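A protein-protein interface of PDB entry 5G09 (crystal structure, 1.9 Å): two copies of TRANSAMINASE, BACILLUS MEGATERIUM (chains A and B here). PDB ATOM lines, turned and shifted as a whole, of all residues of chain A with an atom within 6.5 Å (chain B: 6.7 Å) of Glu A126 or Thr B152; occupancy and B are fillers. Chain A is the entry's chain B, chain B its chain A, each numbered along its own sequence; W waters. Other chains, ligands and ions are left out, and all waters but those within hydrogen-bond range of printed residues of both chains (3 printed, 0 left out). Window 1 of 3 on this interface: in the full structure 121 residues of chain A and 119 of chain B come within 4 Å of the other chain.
The side-chain carboxylate (OE2) of Glu B126 is in hydrogen-bond range of the side-chain hydroxyl (OG1) of Thr B152.
The backbone NH (N) of Gly B153 lies within hydrogen-bond range of the side-chain carboxylate (OE2) of Glu B126, at 3.5 Å.
OG of Ser A122 lies within hydrogen-bond range of N of Trp A151 (3.0 Å).
The backbone carbonyl oxygen of Glu A126 lies close to the side-chain amide oxygen of Asn A130 (3.3 Å).
The side-chain hydroxyl (OG1) of Thr A152 lies within hydrogen-bond range of the side-chain carboxylate (OE2) of Glu A126, 2.6 Å away.
OE2 of Glu A126 lies within hydrogen-bond range of N of Gly A154 (2.7 Å).
Of the 15 printed residues of chain B, 7 touch a printed residue of chain A.
Hydrophobic or aromatic side chains of chain B that line the printed part of chain A: Trp B151.
Of the 19 printed residues of chain A, 7 touch a printed residue of chain B.
Hydrophobic or aromatic side chains of chain A that line the printed part of chain B: Trp A151.
Among the printed residues, no Asp or Glu carboxylate lies within 4 Å of a Lys or Arg side-chain nitrogen of the other chain.
Water W1 bridges OE2 of Glu A123 and NE1 of Trp B151.
Water W2 lies within hydrogen-bond range of the backbone carbonyl oxygen of Trp B151 (2.7 Å), the side-chain amide nitrogen of Asn A130 (2.7 Å) and the backbone NH of Gly B153 (3.5 Å).
Water W3 lies within hydrogen-bond range of the side-chain carboxylate of Glu B123 and the indole nitrogen of Trp A151.
Glu A126 touches three residues of chain B.
Thr B152 touches just these residues of chain A: Glu A123 and Glu A126.
Of the printed residues of chain A, Gly B154 touches Gly A153.
Printed residues of chain B within 4 Å of Gly A153: Glu B126 and Gly B154.
Of the printed residues of chain A, Glu B123 touches Trp A151.
Ala A155 touches none of the printed residues of chain B.
His A149 touches none of the printed residues of chain B.
The nearest residue of chain A that does not touch Thr B152 is Thr A152 (4.6 Å).
The nearest printed residue of chain B that does not touch Thr A152 is Glu B123 (4.1 Å).
Among the printed residues, merely in contact across the chains: Thr A127 with Trp B151, Glu A123 with Trp B151, Trp A151 with Glu B123, Gly A153 with Gly B154, Gly A154 with Gly B153, Thr A152 with Glu B126, Glu A126 with Thr B152, Trp A151 with Glu B126, Glu A126 with Trp B151 and Glu A123 with Thr B152.
OE2 of Glu A123 is in hydrogen-bond range of OG1 of Thr B120 (2.9 Å).
The side-chain carboxylate (OE1) of Glu B126 is in hydrogen-bond range of the backbone NH (N) of Gly A153 (2.7 Å).
N of Gly B153 sits at hydrogen-bond distance from OE1 of Glu A126.
Glu A126 touches Trp B151, and with the chains exchanged Trp A151 touches Glu B126.
Glu A126 touches Thr B152, and with the chains exchanged Thr A152 touches Glu B126.
Glu A126 touches Gly B153, and with the chains exchanged Gly A153 touches Glu B126.
Gly A153 touches Gly B154, and with the chains exchanged Gly A154 touches Gly B153.
Positions printed for both chains: 122, 123, 126, 149, 151, 152, 153, 154, 155 and 156.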
ATOM      1  N   GLY A 121     -12.828  19.935   6.581  1.00  0.00           N
ATOM      2  CA  GLY A 121     -13.293  20.730   7.722  1.00  0.00           C
ATOM      3  C   GLY A 121     -13.123  20.010   9.064  1.00  0.00           C
ATOM      4  O   GLY A 121     -12.805  20.646  10.050  1.00  0.00           O
ATOM      5  N   SER A 122     -13.321  18.695   9.101  1.00  0.00           N
ATOM      6  CA  SER A 122     -13.087  17.939  10.331  1.00  0.00           C
ATOM      7  C   SER A 122     -11.611  17.999  10.709  1.00  0.00           C
ATOM      8  O   SER A 122     -11.281  18.184  11.876  1.00  0.00           O
ATOM      9  CB  SER A 122     -13.555  16.483  10.211  1.00  0.00           C
ATOM     10  OG  SER A 122     -14.957  16.408  10.062  1.00  0.00           O
ATOM     11  N   GLU A 123     -10.719  17.865   9.729  1.00  0.00           N
ATOM     12  CA  GLU A 123      -9.290  18.002  10.028  1.00  0.00           C
ATOM     13  C   GLU A 123      -8.939  19.384  10.578  1.00  0.00           C
ATOM     14  O   GLU A 123      -8.075  19.503  11.481  1.00  0.00           O
ATOM     15  CB  GLU A 123      -8.408  17.623   8.822  1.00  0.00           C
ATOM     16  CG  GLU A 123      -8.365  16.115   8.617  1.00  0.00           C
ATOM     17  CD  GLU A 123      -7.358  15.695   7.571  1.00  0.00           C
ATOM     18  OE1 GLU A 123      -6.927  16.564   6.773  1.00  0.00           O
ATOM     19  OE2 GLU A 123      -6.997  14.501   7.555  1.00  0.00           O
ATOM     20  N   ALA A 124      -9.588  20.429  10.046  1.00  0.00           N
ATOM     21  CA  ALA A 124      -9.290  21.782  10.502  1.00  0.00           C
ATOM     22  C   ALA A 124      -9.741  21.884  11.966  1.00  0.00           C
ATOM     23  O   ALA A 124      -9.039  22.473  12.797  1.00  0.00           O
ATOM     24  CB  ALA A 124     -10.025  22.834   9.661  1.00  0.00           C
ATOM     25  N   VAL A 125     -10.911  21.336  12.269  1.00  0.00           N
ATOM     26  CA  VAL A 125     -11.410  21.363  13.669  1.00  0.00           C
ATOM     27  C   VAL A 125     -10.487  20.537  14.611  1.00  0.00           C
ATOM     28  O   VAL A 125     -10.140  20.996  15.722  1.00  0.00           O
ATOM     29  CB  VAL A 125     -12.895  20.910  13.756  1.00  0.00           C
ATOM     30  CG1 VAL A 125     -13.330  20.592  15.198  1.00  0.00           C
ATOM     31  CG2 VAL A 125     -13.830  21.962  13.131  1.00  0.00           C
ATOM     32  N   GLU A 126     -10.095  19.339  14.192  1.00  0.00           N
ATOM     33  CA  GLU A 126      -9.088  18.537  14.976  1.00  0.00           C
ATOM     34  C   GLU A 126      -7.843  19.387  15.279  1.00  0.00           C
ATOM     35  O   GLU A 126      -7.340  19.400  16.407  1.00  0.00           O
ATOM     36  CB  GLU A 126      -8.637  17.283  14.209  1.00  0.00           C
ATOM     37  CG  GLU A 126      -9.732  16.289  13.831  1.00  0.00           C
ATOM     38  CD  GLU A 126     -10.027  15.306  14.963  1.00  0.00           C
ATOM     39  OE1 GLU A 126      -9.224  15.224  15.909  1.00  0.00           O
ATOM     40  OE2 GLU A 126     -11.054  14.593  14.898  1.00  0.00           O
ATOM     41  N   THR A 127      -7.368  20.110  14.266  1.00  0.00           N
ATOM     42  CA  THR A 127      -6.170  20.943  14.406  1.00  0.00           C
ATOM     43  C   THR A 127      -6.423  22.071  15.446  1.00  0.00           C
ATOM     44  O   THR A 127      -5.594  22.316  16.313  1.00  0.00           O
ATOM     45  CB  THR A 127      -5.730  21.516  13.026  1.00  0.00           C
ATOM     46  OG1 THR A 127      -5.586  20.435  12.077  1.00  0.00           O
ATOM     47  CG2 THR A 127      -4.372  22.203  13.142  1.00  0.00           C
ATOM     48  N   ALA A 128      -7.557  22.748  15.321  1.00  0.00           N
ATOM     49  CA  ALA A 128      -7.914  23.849  16.210  1.00  0.00           C
ATOM     50  C   ALA A 128      -7.983  23.367  17.666  1.00  0.00           C
ATOM     51  O   ALA A 128      -7.490  24.055  18.572  1.00  0.00           O
ATOM     52  CB  ALA A 128      -9.247  24.444  15.802  1.00  0.00           C
ATOM     53  N   LEU A 129      -8.587  22.202  17.889  1.00  0.00           N
ATOM     54  CA  LEU A 129      -8.659  21.651  19.262  1.00  0.00           C
ATOM     55  C   LEU A 129      -7.275  21.384  19.844  1.00  0.00           C
ATOM     56  O   LEU A 129      -7.011  21.735  20.995  1.00  0.00           O
ATOM     57  CB  LEU A 129      -9.529  20.401  19.316  1.00  0.00           C
ATOM     58  CG  LEU A 129     -10.969  20.657  18.892  1.00  0.00           C
ATOM     59  CD1 LEU A 129     -11.642  19.309  18.683  1.00  0.00           C
ATOM     60  CD2 LEU A 129     -11.753  21.512  19.902  1.00  0.00           C
ATOM     61  N   ASN A 130      -6.393  20.790  19.035  1.00  0.00           N
ATOM     62  CA  ASN A 130      -5.032  20.493  19.450  1.00  0.00           C
ATOM     63  C   ASN A 130      -4.268  21.772  19.822  1.00  0.00           C
ATOM     64  O   ASN A 130      -3.620  21.815  20.855  1.00  0.00           O
ATOM     65  CB  ASN A 130      -4.281  19.723  18.331  1.00  0.00           C
ATOM     66  CG  ASN A 130      -4.863  18.338  18.071  1.00  0.00           C
ATOM     67  OD1 ASN A 130      -5.673  17.847  18.857  1.00  0.00           O
ATOM     68  ND2 ASN A 130      -4.448  17.696  16.964  1.00  0.00           N
ATOM     69  N   ILE A 131      -4.344  22.800  18.960  1.00  0.00           N
ATOM     70  CA  ILE A 131      -3.656  24.061  19.217  1.00  0.00           C
ATOM     71  C   ILE A 131      -4.213  24.763  20.463  1.00  0.00           C
ATOM     72  O   ILE A 131      -3.417  25.238  21.289  1.00  0.00           O
ATOM     73  CB  ILE A 131      -3.706  25.026  18.007  1.00  0.00           C
ATOM     74  CG1 ILE A 131      -2.935  24.441  16.793  1.00  0.00           C
ATOM     75  CG2 ILE A 131      -3.067  26.358  18.381  1.00  0.00           C
ATOM     76  CD1 ILE A 131      -3.436  25.039  15.472  1.00  0.00           C
ATOM     77  N   HIS A 149     -19.488  19.935  14.346  1.00  0.00           N
ATOM     78  CA  HIS A 149     -18.136  20.384  14.092  1.00  0.00           C
ATOM     79  C   HIS A 149     -17.357  19.333  13.313  1.00  0.00           C
ATOM     80  O   HIS A 149     -16.149  19.433  13.202  1.00  0.00           O
ATOM     81  CB  HIS A 149     -17.388  20.781  15.401  1.00  0.00           C
ATOM     82  CG  HIS A 149     -17.994  21.974  16.087  1.00  0.00           C
ATOM     83  ND1 HIS A 149     -17.952  23.248  15.548  1.00  0.00           N
ATOM     84  CD2 HIS A 149     -18.719  22.074  17.232  1.00  0.00           C
ATOM     85  CE1 HIS A 149     -18.621  24.078  16.336  1.00  0.00           C
ATOM     86  NE2 HIS A 149     -19.083  23.388  17.371  1.00  0.00           N
ATOM     87  N   TRP A 151     -16.810  14.926  11.931  1.00  0.00           N
ATOM     88  CA  TRP A 151     -17.149  13.514  12.205  1.00  0.00           C
ATOM     89  C   TRP A 151     -15.978  12.696  12.715  1.00  0.00           C
ATOM     90  O   TRP A 151     -16.186  11.572  13.191  1.00  0.00           O
ATOM     91  CB  TRP A 151     -17.709  12.846  10.934  1.00  0.00           C
ATOM     92  CG  TRP A 151     -16.665  12.757   9.849  1.00  0.00           C
ATOM     93  CD1 TRP A 151     -16.384  13.692   8.879  1.00  0.00           C
ATOM     94  CD2 TRP A 151     -15.764  11.671   9.637  1.00  0.00           C
ATOM     95  NE1 TRP A 151     -15.326  13.256   8.100  1.00  0.00           N
ATOM     96  CE2 TRP A 151     -14.944  12.011   8.535  1.00  0.00           C
ATOM     97  CE3 TRP A 151     -15.566  10.424  10.280  1.00  0.00           C
ATOM     98  CZ2 TRP A 151     -13.946  11.146   8.046  1.00  0.00           C
ATOM     99  CZ3 TRP A 151     -14.531   9.584   9.817  1.00  0.00           C
ATOM    100  CH2 TRP A 151     -13.747   9.953   8.705  1.00  0.00           C
ATOM    101  N   THR A 152     -14.752  13.208  12.566  1.00  0.00           N
ATOM    102  CA  THR A 152     -13.585  12.443  13.002  1.00  0.00           C
ATOM    103  C   THR A 152     -13.527  12.435  14.530  1.00  0.00           C
ATOM    104  O   THR A 152     -14.249  13.197  15.179  1.00  0.00           O
ATOM    105  CB  THR A 152     -12.291  12.976  12.388  1.00  0.00           C
ATOM    106  OG1 THR A 152     -12.227  14.396  12.584  1.00  0.00           O
ATOM    107  CG2 THR A 152     -12.255  12.663  10.865  1.00  0.00           C
ATOM    108  N   GLY A 153     -12.718  11.551  15.109  1.00  0.00           N
ATOM    109  CA  GLY A 153     -12.738  11.315  16.561  1.00  0.00           C
ATOM    110  C   GLY A 153     -12.762  12.551  17.462  1.00  0.00           C
ATOM    111  O   GLY A 153     -13.627  12.646  18.337  1.00  0.00           O
ATOM    112  N   GLY A 154     -11.825  13.491  17.267  1.00  0.00           N
ATOM    113  CA  GLY A 154     -11.788  14.725  18.046  1.00  0.00           C
ATOM    114  C   GLY A 154     -12.909  15.702  17.736  1.00  0.00           C
ATOM    115  O   GLY A 154     -13.555  16.242  18.638  1.00  0.00           O
ATOM    116  N   ALA A 155     -13.157  15.933  16.449  1.00  0.00           N
ATOM    117  CA  ALA A 155     -14.214  16.867  16.034  1.00  0.00           C
ATOM    118  C   ALA A 155     -15.611  16.358  16.495  1.00  0.00           C
ATOM    119  O   ALA A 155     -16.500  17.155  16.845  1.00  0.00           O
ATOM    120  CB  ALA A 155     -14.165  17.066  14.517  1.00  0.00           C
ATOM    121  N   ALA A 156     -15.796  15.033  16.502  1.00  0.00           N
ATOM    122  CA  ALA A 156     -17.052  14.445  16.934  1.00  0.00           C
ATOM    123  C   ALA A 156     -17.311  14.675  18.429  1.00  0.00           C
ATOM    124  O   ALA A 156     -18.462  14.852  18.817  1.00  0.00           O
ATOM    125  CB  ALA A 156     -17.078  12.956  16.628  1.00  0.00           C
ATOM    126  N   THR A 295     -11.881  27.877  12.113  1.00  0.00           N
ATOM    127  CA  THR A 295     -11.719  26.700  11.270  1.00  0.00           C
ATOM    128  C   THR A 295     -12.452  26.931   9.957  1.00  0.00           C
ATOM    129  O   THR A 295     -13.497  27.614   9.937  1.00  0.00           O
ATOM    130  CB  THR A 295     -12.222  25.428  11.959  1.00  0.00           C
ATOM    131  OG1 THR A 295     -13.542  25.658  12.453  1.00  0.00           O
ATOM    132  CG2 THR A 295     -11.311  25.074  13.159  1.00  0.00           C
ATOM    133  N   THR B 120      -8.310  11.314   3.263  1.00  0.00           N
ATOM    134  CA  THR B 120      -6.974  11.158   3.834  1.00  0.00           C
ATOM    135  C   THR B 120      -6.820   9.809   4.501  1.00  0.00           C
ATOM    136  O   THR B 120      -7.795   9.120   4.764  1.00  0.00           O
ATOM    137  CB  THR B 120      -6.625  12.251   4.889  1.00  0.00           C
ATOM    138  OG1 THR B 120      -7.410  12.068   6.082  1.00  0.00           O
ATOM    139  CG2 THR B 120      -6.846  13.655   4.335  1.00  0.00           C
ATOM    140  N   SER B 122      -5.694   9.268   7.593  1.00  0.00           N
ATOM    141  CA  SER B 122      -6.223   9.360   8.980  1.00  0.00           C
ATOM    142  C   SER B 122      -7.747   9.215   8.973  1.00  0.00           C
ATOM    143  O   SER B 122      -8.335   8.551   9.830  1.00  0.00           O
ATOM    144  CB  SER B 122      -5.835  10.694   9.643  1.00  0.00           C
ATOM    145  OG  SER B 122      -4.448  10.835   9.807  1.00  0.00           O
ATOM    146  N   GLU B 123      -8.411   9.853   8.004  1.00  0.00           N
ATOM    147  CA  GLU B 123      -9.871   9.688   7.850  1.00  0.00           C
ATOM    148  C   GLU B 123     -10.219   8.227   7.573  1.00  0.00           C
ATOM    149  O   GLU B 123     -11.225   7.720   8.047  1.00  0.00           O
ATOM    150  CB  GLU B 123     -10.453  10.644   6.773  1.00  0.00           C
ATOM    151  CG  GLU B 123     -10.460  12.100   7.243  1.00  0.00           C
ATOM    152  CD  GLU B 123     -11.298  13.040   6.384  1.00  0.00           C
ATOM    153  OE1 GLU B 123     -11.617  12.673   5.235  1.00  0.00           O
ATOM    154  OE2 GLU B 123     -11.660  14.154   6.877  1.00  0.00           O
ATOM    155  N   GLU B 126      -9.937   6.462  10.893  1.00  0.00           N
ATOM    156  CA  GLU B 126     -11.103   6.847  11.719  1.00  0.00           C
ATOM    157  C   GLU B 126     -12.340   6.032  11.321  1.00  0.00           C
ATOM    158  O   GLU B 126     -13.031   5.487  12.175  1.00  0.00           O
ATOM    159  CB  GLU B 126     -11.408   8.335  11.546  1.00  0.00           C
ATOM    160  CG  GLU B 126     -10.301   9.271  12.002  1.00  0.00           C
ATOM    161  CD  GLU B 126     -10.387   9.707  13.458  1.00  0.00           C
ATOM    162  OE1 GLU B 126     -11.373   9.396  14.153  1.00  0.00           O
ATOM    163  OE2 GLU B 126      -9.452  10.429  13.906  1.00  0.00           O
ATOM    164  N   TYR B 148       2.089   3.759  13.676  1.00  0.00           N
ATOM    165  CA  TYR B 148       1.588   5.062  13.242  1.00  0.00           C
ATOM    166  C   TYR B 148       0.344   4.823  12.383  1.00  0.00           C
ATOM    167  O   TYR B 148       0.418   4.144  11.326  1.00  0.00           O
ATOM    168  CB  TYR B 148       2.655   5.865  12.451  1.00  0.00           C
ATOM    169  CG  TYR B 148       2.126   7.278  12.196  1.00  0.00           C
ATOM    170  CD1 TYR B 148       2.185   8.239  13.201  1.00  0.00           C
ATOM    171  CD2 TYR B 148       1.492   7.615  10.982  1.00  0.00           C
ATOM    172  CE1 TYR B 148       1.648   9.494  13.018  1.00  0.00           C
ATOM    173  CE2 TYR B 148       0.964   8.894  10.786  1.00  0.00           C
ATOM    174  CZ  TYR B 148       1.049   9.833  11.811  1.00  0.00           C
ATOM    175  OH  TYR B 148       0.511  11.118  11.650  1.00  0.00           O
ATOM    176  N   HIS B 149      -0.807   5.336  12.827  1.00  0.00           N
ATOM    177  CA  HIS B 149      -2.021   5.186  12.049  1.00  0.00           C
ATOM    178  C   HIS B 149      -2.722   6.526  11.723  1.00  0.00           C
ATOM    179  O   HIS B 149      -3.888   6.533  11.374  1.00  0.00           O
ATOM    180  CB  HIS B 149      -2.991   4.257  12.794  1.00  0.00           C
ATOM    181  CG  HIS B 149      -2.460   2.858  12.994  1.00  0.00           C
ATOM    182  ND1 HIS B 149      -2.291   1.970  11.947  1.00  0.00           N
ATOM    183  CD2 HIS B 149      -2.047   2.203  14.111  1.00  0.00           C
ATOM    184  CE1 HIS B 149      -1.792   0.831  12.409  1.00  0.00           C
ATOM    185  NE2 HIS B 149      -1.642   0.938  13.721  1.00  0.00           N
ATOM    186  N   GLY B 150      -2.017   7.646  11.877  1.00  0.00           N
ATOM    187  CA  GLY B 150      -2.591   8.968  11.579  1.00  0.00           C
ATOM    188  C   GLY B 150      -2.591   9.888  12.788  1.00  0.00           C
ATOM    189  O   GLY B 150      -2.068   9.525  13.864  1.00  0.00           O
ATOM    190  N   TRP B 151      -3.162  11.085  12.611  1.00  0.00           N
ATOM    191  CA  TRP B 151      -2.938  12.180  13.554  1.00  0.00           C
ATOM    192  C   TRP B 151      -4.228  12.730  14.118  1.00  0.00           C
ATOM    193  O   TRP B 151      -4.203  13.415  15.123  1.00  0.00           O
ATOM    194  CB  TRP B 151      -2.163  13.331  12.898  1.00  0.00           C
ATOM    195  CG  TRP B 151      -2.959  14.004  11.786  1.00  0.00           C
ATOM    196  CD1 TRP B 151      -2.991  13.632  10.466  1.00  0.00           C
ATOM    197  CD2 TRP B 151      -3.850  15.112  11.916  1.00  0.00           C
ATOM    198  NE1 TRP B 151      -3.835  14.446   9.773  1.00  0.00           N
ATOM    199  CE2 TRP B 151      -4.372  15.377  10.629  1.00  0.00           C
ATOM    200  CE3 TRP B 151      -4.223  15.941  12.989  1.00  0.00           C
ATOM    201  CZ2 TRP B 151      -5.256  16.439  10.371  1.00  0.00           C
ATOM    202  CZ3 TRP B 151      -5.139  16.997  12.744  1.00  0.00           C
ATOM    203  CH2 TRP B 151      -5.646  17.228  11.442  1.00  0.00           C
ATOM    204  N   THR B 152      -5.341  12.524  13.429  1.00  0.00           N
ATOM    205  CA  THR B 152      -6.631  13.023  13.935  1.00  0.00           C
ATOM    206  C   THR B 152      -7.022  12.270  15.227  1.00  0.00           C
ATOM    207  O   THR B 152      -6.427  11.245  15.560  1.00  0.00           O
ATOM    208  CB  THR B 152      -7.735  12.893  12.870  1.00  0.00           C
ATOM    209  OG1 THR B 152      -7.785  11.532  12.423  1.00  0.00           O
ATOM    210  CG2 THR B 152      -7.405  13.800  11.661  1.00  0.00           C
ATOM    211  N   GLY B 153      -7.996  12.809  15.967  1.00  0.00           N
ATOM    212  CA  GLY B 153      -8.353  12.317  17.316  1.00  0.00           C
ATOM    213  C   GLY B 153      -8.492  10.814  17.503  1.00  0.00           C
ATOM    214  O   GLY B 153      -7.834  10.259  18.373  1.00  0.00           O
ATOM    215  N   GLY B 154      -9.318  10.133  16.704  1.00  0.00           N
ATOM    216  CA  GLY B 154      -9.439   8.688  16.842  1.00  0.00           C
ATOM    217  C   GLY B 154      -8.227   7.917  16.338  1.00  0.00           C
ATOM    218  O   GLY B 154      -7.720   7.002  17.013  1.00  0.00           O
ATOM    219  N   ALA B 155      -7.764   8.267  15.131  1.00  0.00           N
ATOM    220  CA  ALA B 155      -6.561   7.659  14.558  1.00  0.00           C
ATOM    221  C   ALA B 155      -5.338   7.806  15.459  1.00  0.00           C
ATOM    222  O   ALA B 155      -4.537   6.875  15.522  1.00  0.00           O
ATOM    223  CB  ALA B 155      -6.252   8.231  13.172  1.00  0.00           C
ATOM    224  N   ALA B 156      -5.165   8.963  16.109  1.00  0.00           N
ATOM    225  CA  ALA B 156      -4.038   9.154  17.048  1.00  0.00           C
ATOM    226  C   ALA B 156      -4.080   8.211  18.268  1.00  0.00           C
ATOM    227  O   ALA B 156      -3.027   7.885  18.847  1.00  0.00           O
ATOM    228  CB  ALA B 156      -3.982  10.603  17.547  1.00  0.00           C
ATOM    229  N   THR B 157      -5.286   7.814  18.706  1.00  0.00           N
ATOM    230  CA  THR B 157      -5.341   6.941  19.881  1.00  0.00           C
ATOM    231  C   THR B 157      -4.592   5.617  19.589  1.00  0.00           C
ATOM    232  O   THR B 157      -4.050   5.003  20.515  1.00  0.00           O
ATOM    233  CB  THR B 157      -6.785   6.643  20.356  1.00  0.00           C
ATOM    234  OG1 THR B 157      -7.446   5.886  19.351  1.00  0.00           O
ATOM    235  CG2 THR B 157      -7.628   7.952  20.667  1.00  0.00           C
ATOM    236  N   SER B 166       1.661  14.816  17.621  1.00  0.00           N
ATOM    237  CA  SER B 166       1.180  16.221  17.526  1.00  0.00           C
ATOM    238  C   SER B 166       1.416  17.074  18.761  1.00  0.00           C
ATOM    239  O   SER B 166       0.720  18.075  18.978  1.00  0.00           O
ATOM    240  CB  SER B 166      -0.286  16.293  17.118  1.00  0.00           C
ATOM    241  OG  SER B 166      -0.402  15.700  15.829  1.00  0.00           O
HETATM  242  O   HOH W   1      -4.465  13.822   7.075  1.00  0.00           O
HETATM  243  O   HOH W   2      -5.626  15.250  16.571  1.00  0.00           O
HETATM  244  O   HOH W   3     -14.219  15.073   6.167  1.00  0.00           O
